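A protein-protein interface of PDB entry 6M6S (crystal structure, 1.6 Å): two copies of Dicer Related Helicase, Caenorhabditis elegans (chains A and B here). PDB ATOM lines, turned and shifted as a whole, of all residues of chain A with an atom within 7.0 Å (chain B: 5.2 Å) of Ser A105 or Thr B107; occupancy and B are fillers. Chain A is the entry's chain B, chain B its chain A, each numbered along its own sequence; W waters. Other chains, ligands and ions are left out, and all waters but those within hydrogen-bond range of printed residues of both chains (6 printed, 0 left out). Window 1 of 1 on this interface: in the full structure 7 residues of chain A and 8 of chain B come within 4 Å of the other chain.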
ATOM      1  N   TYR A  10      25.242 -14.557  20.855  1.00  0.00           N
ATOM      2  CA  TYR A  10      24.702 -15.820  21.259  1.00  0.00           C
ATOM      3  C   TYR A  10      24.684 -15.952  22.744  1.00  0.00           C
ATOM      4  O   TYR A  10      25.568 -15.429  23.435  1.00  0.00           O
ATOM      5  CB  TYR A  10      25.558 -16.994  20.679  1.00  0.00           C
ATOM      6  CG  TYR A  10      25.331 -17.184  19.199  1.00  0.00           C
ATOM      7  CD1 TYR A  10      25.862 -16.296  18.276  1.00  0.00           C
ATOM      8  CD2 TYR A  10      24.606 -18.250  18.740  1.00  0.00           C
ATOM      9  CE1 TYR A  10      25.666 -16.443  16.911  1.00  0.00           C
ATOM     10  CE2 TYR A  10      24.388 -18.401  17.369  1.00  0.00           C
ATOM     11  CZ  TYR A  10      24.951 -17.522  16.478  1.00  0.00           C
ATOM     12  OH  TYR A  10      24.762 -17.673  15.135  1.00  0.00           O
ATOM     13  N   THR A  96      25.360 -25.424  24.804  1.00  0.00           N
ATOM     14  CA  THR A  96      24.504 -25.196  23.648  1.00  0.00           C
ATOM     15  C   THR A  96      24.569 -23.703  23.395  1.00  0.00           C
ATOM     16  O   THR A  96      24.427 -22.876  24.327  1.00  0.00           O
ATOM     17  CB  THR A  96      23.084 -25.629  23.934  1.00  0.00           C
ATOM     18  OG1 THR A  96      23.075 -27.068  24.088  1.00  0.00           O
ATOM     19  CG2 THR A  96      22.171 -25.377  22.727  1.00  0.00           C
ATOM     20  N   PHE A  97      24.788 -23.295  22.138  1.00  0.00           N
ATOM     21  CA  PHE A  97      24.785 -21.884  21.766  1.00  0.00           C
ATOM     22  C   PHE A  97      23.416 -21.517  21.224  1.00  0.00           C
ATOM     23  O   PHE A  97      22.878 -22.224  20.367  1.00  0.00           O
ATOM     24  CB  PHE A  97      25.848 -21.629  20.714  1.00  0.00           C
ATOM     25  CG  PHE A  97      27.233 -21.955  21.197  1.00  0.00           C
ATOM     26  CD1 PHE A  97      27.996 -21.005  21.835  1.00  0.00           C
ATOM     27  CD2 PHE A  97      27.747 -23.214  21.020  1.00  0.00           C
ATOM     28  CE1 PHE A  97      29.267 -21.339  22.283  1.00  0.00           C
ATOM     29  CE2 PHE A  97      29.009 -23.561  21.481  1.00  0.00           C
ATOM     30  CZ  PHE A  97      29.771 -22.566  22.101  1.00  0.00           C
ATOM     31  N   VAL A  98      22.823 -20.437  21.764  1.00  0.00           N
ATOM     32  CA  VAL A  98      21.466 -20.105  21.298  1.00  0.00           C
ATOM     33  C   VAL A  98      21.464 -18.695  20.717  1.00  0.00           C
ATOM     34  O   VAL A  98      21.950 -17.756  21.387  1.00  0.00           O
ATOM     35  CB  VAL A  98      20.488 -20.171  22.464  1.00  0.00           C
ATOM     36  CG1 VAL A  98      19.129 -19.549  22.049  1.00  0.00           C
ATOM     37  CG2 VAL A  98      20.400 -21.611  23.019  1.00  0.00           C
ATOM     38  N   GLN A  99      20.901 -18.527  19.522  1.00  0.00           N
ATOM     39  CA  GLN A  99      20.662 -17.191  18.969  1.00  0.00           C
ATOM     40  C   GLN A  99      19.197 -16.891  19.209  1.00  0.00           C
ATOM     41  O   GLN A  99      18.324 -17.385  18.519  1.00  0.00           O
ATOM     42  CB  GLN A  99      20.977 -17.135  17.470  1.00  0.00           C
ATOM     43  CG  GLN A  99      21.572 -15.775  17.057  1.00  0.00           C
ATOM     44  CD  GLN A  99      20.632 -14.600  17.379  1.00  0.00           C
ATOM     45  OE1 GLN A  99      19.463 -14.623  16.999  1.00  0.00           O
ATOM     46  NE2 GLN A  99      21.138 -13.591  18.094  1.00  0.00           N
ATOM     47  N   ASP A 102      16.887 -15.477  16.120  1.00  0.00           N
ATOM     48  CA  ASP A 102      16.694 -16.485  15.084  1.00  0.00           C
ATOM     49  C   ASP A 102      15.971 -17.748  15.566  1.00  0.00           C
ATOM     50  O   ASP A 102      15.657 -18.621  14.736  1.00  0.00           O
ATOM     51  CB  ASP A 102      18.048 -16.912  14.501  1.00  0.00           C
ATOM     52  CG  ASP A 102      18.809 -15.754  13.882  1.00  0.00           C
ATOM     53  OD1 ASP A 102      18.176 -14.722  13.543  1.00  0.00           O
ATOM     54  OD2 ASP A 102      20.052 -15.872  13.742  1.00  0.00           O
ATOM     55  N   TYR A 103      15.738 -17.867  16.866  1.00  0.00           N
ATOM     56  CA  TYR A 103      15.181 -19.106  17.410  1.00  0.00           C
ATOM     57  C   TYR A 103      16.034 -20.300  16.961  1.00  0.00           C
ATOM     58  O   TYR A 103      15.492 -21.284  16.463  1.00  0.00           O
ATOM     59  CB  TYR A 103      13.748 -19.293  16.975  1.00  0.00           C
ATOM     60  CG  TYR A 103      12.890 -18.178  17.525  1.00  0.00           C
ATOM     61  CD1 TYR A 103      12.496 -18.200  18.854  1.00  0.00           C
ATOM     62  CD2 TYR A 103      12.540 -17.087  16.752  1.00  0.00           C
ATOM     63  CE1 TYR A 103      11.725 -17.178  19.399  1.00  0.00           C
ATOM     64  CE2 TYR A 103      11.770 -16.043  17.292  1.00  0.00           C
ATOM     65  CZ  TYR A 103      11.365 -16.107  18.617  1.00  0.00           C
ATOM     66  OH  TYR A 103      10.597 -15.095  19.175  1.00  0.00           O
ATOM     67  N   SER A 104      17.350 -20.188  17.124  1.00  0.00           N
ATOM     68  CA  SER A 104      18.213 -21.275  16.632  1.00  0.00           C
ATOM     69  C   SER A 104      19.123 -21.703  17.723  1.00  0.00           C
ATOM     70  O   SER A 104      19.493 -20.905  18.590  1.00  0.00           O
ATOM     71  CB  SER A 104      19.065 -20.773  15.489  1.00  0.00           C
ATOM     72  OG  SER A 104      19.968 -19.791  15.995  1.00  0.00           O
ATOM     73  N   SER A 105      19.475 -22.981  17.742  1.00  0.00           N
ATOM     74  CA  SER A 105      20.490 -23.385  18.686  1.00  0.00           C
ATOM     75  C   SER A 105      21.467 -24.327  18.025  1.00  0.00           C
ATOM     76  O   SER A 105      21.122 -24.949  17.022  1.00  0.00           O
ATOM     77  CB  SER A 105      19.904 -24.012  19.935  1.00  0.00           C
ATOM     78  OG  SER A 105      19.389 -25.263  19.605  1.00  0.00           O
ATOM     79  N   MET A 106      22.683 -24.396  18.589  1.00  0.00           N
ATOM     80  CA  MET A 106      23.760 -25.176  17.919  1.00  0.00           C
ATOM     81  C   MET A 106      24.671 -25.821  18.950  1.00  0.00           C
ATOM     82  O   MET A 106      24.997 -25.242  20.005  1.00  0.00           O
ATOM     83  CB  MET A 106      24.616 -24.235  17.053  1.00  0.00           C
ATOM     84  CG  MET A 106      23.868 -23.501  15.914  1.00  0.00           C
ATOM     85  SD  MET A 106      23.281 -21.940  16.682  1.00  0.00           S
ATOM     86  CE  MET A 106      22.918 -21.115  15.170  1.00  0.00           C
ATOM     87  N   THR A 107      25.144 -27.021  18.666  1.00  0.00           N
ATOM     88  CA  THR A 107      26.228 -27.596  19.449  1.00  0.00           C
ATOM     89  C   THR A 107      27.404 -27.748  18.514  1.00  0.00           C
ATOM     90  O   THR A 107      27.183 -27.944  17.276  1.00  0.00           O
ATOM     91  CB  THR A 107      25.903 -28.936  20.130  1.00  0.00           C
ATOM     92  OG1 THR A 107      25.667 -29.979  19.147  1.00  0.00           O
ATOM     93  CG2 THR A 107      24.663 -28.858  21.072  1.00  0.00           C
ATOM     94  N   LYS A 108      28.615 -27.601  19.073  1.00  0.00           N
ATOM     95  CA  LYS A 108      29.849 -27.584  18.273  1.00  0.00           C
ATOM     96  C   LYS A 108      30.898 -28.495  18.946  1.00  0.00           C
ATOM     97  O   LYS A 108      30.879 -28.673  20.172  1.00  0.00           O
ATOM     98  CB  LYS A 108      30.375 -26.144  18.204  1.00  0.00           C
ATOM     99  CG  LYS A 108      29.428 -25.192  17.420  1.00  0.00           C
ATOM    100  CD  LYS A 108      29.364 -25.628  15.947  1.00  0.00           C
ATOM    101  CE  LYS A 108      28.350 -24.766  15.144  1.00  0.00           C
ATOM    102  NZ  LYS A 108      28.143 -25.251  13.736  1.00  0.00           N
ATOM    103  N   LEU A 118      29.847 -19.435  14.015  1.00  0.00           N
ATOM    104  CA  LEU A 118      28.861 -18.710  14.830  1.00  0.00           C
ATOM    105  C   LEU A 118      29.266 -17.272  15.129  1.00  0.00           C
ATOM    106  O   LEU A 118      28.519 -16.330  14.834  1.00  0.00           O
ATOM    107  CB  LEU A 118      28.570 -19.440  16.161  1.00  0.00           C
ATOM    108  CG  LEU A 118      28.083 -20.915  16.054  1.00  0.00           C
ATOM    109  CD1 LEU A 118      27.760 -21.523  17.425  1.00  0.00           C
ATOM    110  CD2 LEU A 118      26.822 -20.971  15.143  1.00  0.00           C
ATOM    111  N   LEU B  95      23.205 -30.952   8.389  1.00  0.00           N
ATOM    112  CA  LEU B  95      21.764 -30.891   8.623  1.00  0.00           C
ATOM    113  C   LEU B  95      21.347 -29.802   9.560  1.00  0.00           C
ATOM    114  O   LEU B  95      22.080 -29.477  10.510  1.00  0.00           O
ATOM    115  CB  LEU B  95      21.280 -32.222   9.198  1.00  0.00           C
ATOM    116  CG  LEU B  95      21.489 -33.400   8.203  1.00  0.00           C
ATOM    117  CD1 LEU B  95      21.073 -34.693   8.984  1.00  0.00           C
ATOM    118  CD2 LEU B  95      20.642 -33.235   6.925  1.00  0.00           C
ATOM    119  N   THR B  96      20.140 -29.304   9.312  1.00  0.00           N
ATOM    120  CA  THR B  96      19.455 -28.492  10.346  1.00  0.00           C
ATOM    121  C   THR B  96      18.175 -29.264  10.701  1.00  0.00           C
ATOM    122  O   THR B  96      17.501 -29.824   9.828  1.00  0.00           O
ATOM    123  CB  THR B  96      19.106 -27.145   9.792  1.00  0.00           C
ATOM    124  OG1 THR B  96      20.326 -26.427   9.528  1.00  0.00           O
ATOM    125  CG2 THR B  96      18.339 -26.323  10.885  1.00  0.00           C
ATOM    126  N   PHE B  97      17.820 -29.330  11.969  1.00  0.00           N
ATOM    127  CA  PHE B  97      16.631 -30.052  12.404  1.00  0.00           C
ATOM    128  C   PHE B  97      15.552 -29.085  12.800  1.00  0.00           C
ATOM    129  O   PHE B  97      15.820 -28.140  13.540  1.00  0.00           O
ATOM    130  CB  PHE B  97      16.980 -30.926  13.635  1.00  0.00           C
ATOM    131  CG  PHE B  97      18.002 -32.000  13.328  1.00  0.00           C
ATOM    132  CD1 PHE B  97      19.386 -31.743  13.411  1.00  0.00           C
ATOM    133  CD2 PHE B  97      17.573 -33.272  12.956  1.00  0.00           C
ATOM    134  CE1 PHE B  97      20.308 -32.743  13.106  1.00  0.00           C
ATOM    135  CE2 PHE B  97      18.488 -34.280  12.635  1.00  0.00           C
ATOM    136  CZ  PHE B  97      19.863 -34.053  12.742  1.00  0.00           C
ATOM    137  N   SER B 105      15.041 -23.938  15.282  1.00  0.00           N
ATOM    138  CA  SER B 105      15.839 -24.840  14.478  1.00  0.00           C
ATOM    139  C   SER B 105      17.060 -25.223  15.316  1.00  0.00           C
ATOM    140  O   SER B 105      17.480 -24.435  16.212  1.00  0.00           O
ATOM    141  CB  SER B 105      16.294 -24.166  13.203  1.00  0.00           C
ATOM    142  OG  SER B 105      17.023 -23.027  13.553  1.00  0.00           O
ATOM    143  N   MET B 106      17.622 -26.392  15.028  1.00  0.00           N
ATOM    144  CA  MET B 106      18.732 -26.907  15.854  1.00  0.00           C
ATOM    145  C   MET B 106      19.763 -27.500  14.908  1.00  0.00           C
ATOM    146  O   MET B 106      19.457 -28.240  13.996  1.00  0.00           O
ATOM    147  CB  MET B 106      18.301 -28.053  16.773  1.00  0.00           C
ATOM    148  CG  MET B 106      17.478 -27.706  18.007  1.00  0.00           C
ATOM    149  SD  MET B 106      15.805 -27.232  17.496  1.00  0.00           S
ATOM    150  CE  MET B 106      15.089 -28.729  16.907  1.00  0.00           C
ATOM    151  N   THR B 107      21.025 -27.214  15.170  1.00  0.00           N
ATOM    152  CA  THR B 107      22.094 -28.003  14.554  1.00  0.00           C
ATOM    153  C   THR B 107      22.919 -28.713  15.633  1.00  0.00           C
ATOM    154  O   THR B 107      23.065 -28.167  16.753  1.00  0.00           O
ATOM    155  CB  THR B 107      22.990 -27.171  13.620  1.00  0.00           C
ATOM    156  OG1 THR B 107      23.698 -26.185  14.350  1.00  0.00           O
ATOM    157  CG2 THR B 107      22.186 -26.408  12.598  1.00  0.00           C
ATOM    158  N   LYS B 108      23.414 -29.899  15.311  1.00  0.00           N
ATOM    159  CA  LYS B 108      24.160 -30.705  16.278  1.00  0.00           C
ATOM    160  C   LYS B 108      25.493 -31.162  15.703  1.00  0.00           C
ATOM    161  O   LYS B 108      25.587 -31.540  14.536  1.00  0.00           O
ATOM    162  CB  LYS B 108      23.336 -31.954  16.682  1.00  0.00           C
ATOM    163  CG  LYS B 108      21.932 -31.619  17.223  1.00  0.00           C
ATOM    164  CD  LYS B 108      22.059 -30.862  18.595  1.00  0.00           C
ATOM    165  CE  LYS B 108      20.612 -30.738  19.133  1.00  0.00           C
ATOM    166  NZ  LYS B 108      20.663 -29.877  20.434  1.00  0.00           N
ATOM    167  N   ALA B 109      26.505 -31.147  16.558  1.00  0.00           N
ATOM    168  CA  ALA B 109      27.841 -31.554  16.142  1.00  0.00           C
ATOM    169  C   ALA B 109      27.956 -33.067  15.983  1.00  0.00           C
ATOM    170  O   ALA B 109      28.838 -33.539  15.246  1.00  0.00           O
ATOM    171  CB  ALA B 109      28.872 -31.035  17.144  1.00  0.00           C
HETATM  172  O   HOH W   1      20.126 -23.908  14.284  1.00  0.00           O
HETATM  173  O   HOH W   2      14.505 -21.072  13.598  1.00  0.00           O
HETATM  174  O   HOH W   3      16.387 -23.926  18.885  1.00  0.00           O
HETATM  175  O   HOH W   4      26.101 -27.351  14.901  1.00  0.00           O
HETATM  176  O   HOH W   5      25.490 -24.402  12.873  1.00  0.00           O
HETATM  177  O   HOH W   6      21.296 -27.494  19.033  1.00  0.00           O
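The backbone NH (N) of Ser B105 is in hydrogen-bond range of the backbone carbonyl oxygen (O) of Tyr A103, at 2.9 Å.
The backbone carbonyl oxygen (O) of Ser B105 lies within hydrogen-bond range of the backbone NH (N) of Ser A105 (2.9 Å).
N of Thr B107 lies within hydrogen-bond range of O of Ser A105 (2.9 Å).
O of Thr B107 sits at hydrogen-bond distance from N of Thr A107.
The backbone NH (N) of Ala B109 is in hydrogen-bond range of the side-chain hydroxyl (OG1) of Thr A107.
O of Met B106 lies within hydrogen-bond range of N of Phe B97 (2.8 Å).
O of Phe A97 sits at hydrogen-bond distance from N of Met A106.
O of Ser A104 sits at hydrogen-bond distance from N of Gln A99, at 2.9 Å.
CA of Ser A104 touches O of Ser B105, at 3.3 Å.
Ser A105 touches Met B106.
CG of Met A106 touches OG1 of Thr B107, 3.1 Å away.
Thr A107 touches Lys B108 (OG1 to CA, 3.3 Å).
Ala B109 touches Lys A108.
Ser A105 touches just these residues of chain B: Ser B105 (2.9 Å), Met B106 (3.3 Å) and Thr B107 (2.9 Å).
Of the printed residues of chain B, Met A106 touches Thr B107 (3.1 Å).
Of the printed residues of chain A, Met B106 touches Ser A105 (3.3 Å).
Printed residues of chain B within 4 Å of Lys A108: Ala B109.
Of the printed residues of chain B, Tyr A103 touches Ser B105.
Printed residues of chain B within 4 Å of Ser A104: Ser B105 (3.3 Å).
Gln A99 touches none of the printed residues of chain B.
The nearest residue of chain B that does not touch Ser A105 is Lys B108 (4.9 Å).
The nearest residue of chain A that does not touch Thr B107 is Lys A108 (4.6 Å).
The nearest printed residue of chain B that does not touch Lys A108 is Thr B107 (4.6 Å).
Hydrophobic or aromatic side chains of chain A that line the printed part of chain B: Met A106.
Of the 8 printed residues of chain B, 5 touch a printed residue of chain A.
Printed residues of chain B that touch a printed residue of chain A: Ser B105, Met B106, Thr B107, Lys B108 and Ala B109.
Hydrophobic or aromatic side chains of chain B within 4 Å of the printed part of chain A: Met B106 and Ala B109.
Among the printed residues, no Asp or Glu carboxylate lies within 4 Å of a Lys or Arg side-chain nitrogen of the other chain.
Ser A105 touches Met B106, but with the chains exchanged Met A106 does not touch Ser B105 (5.7 Å).
Ser A105 touches Thr B107, but with the chains exchanged Thr A107 does not touch Ser B105 (8.5 Å).
Met A106 touches Thr B107, but with the chains exchanged Thr A107 does not touch Met B106 (6.6 Å).
Thr A107 touches Lys B108, but with the chains exchanged Lys A108 does not touch Thr B107 (4.6 Å).
Water W4 lies within hydrogen-bond range of O of Thr A107, OG1 of Thr B107 and NZ of Lys A108.
Water W6 lies within hydrogen-bond range of NZ of Lys B108 (2.8 Å), O of Thr B107 (3.0 Å), OG of Ser A105 (3.0 Å) and N of Met A106 (3.4 Å).
Water W5 bridges NZ of Lys A108 (2.9 Å) and OG1 of Thr B107 (2.9 Å).
Water W3 lies within hydrogen-bond range of O of Ser B105, OG of Ser A105 and SD of Met B106.
Water W2 lies within hydrogen-bond range of O of Asp A102 (2.9 Å), O of Tyr A103 (3.0 Å) and OG of Ser B105 (3.2 Å).
Water W1 lies within hydrogen-bond range of the backbone carbonyl oxygen (O) of Ser A105 (3.1 Å) and the side-chain hydroxyl (OG) of Ser B105 (3.3 Å).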
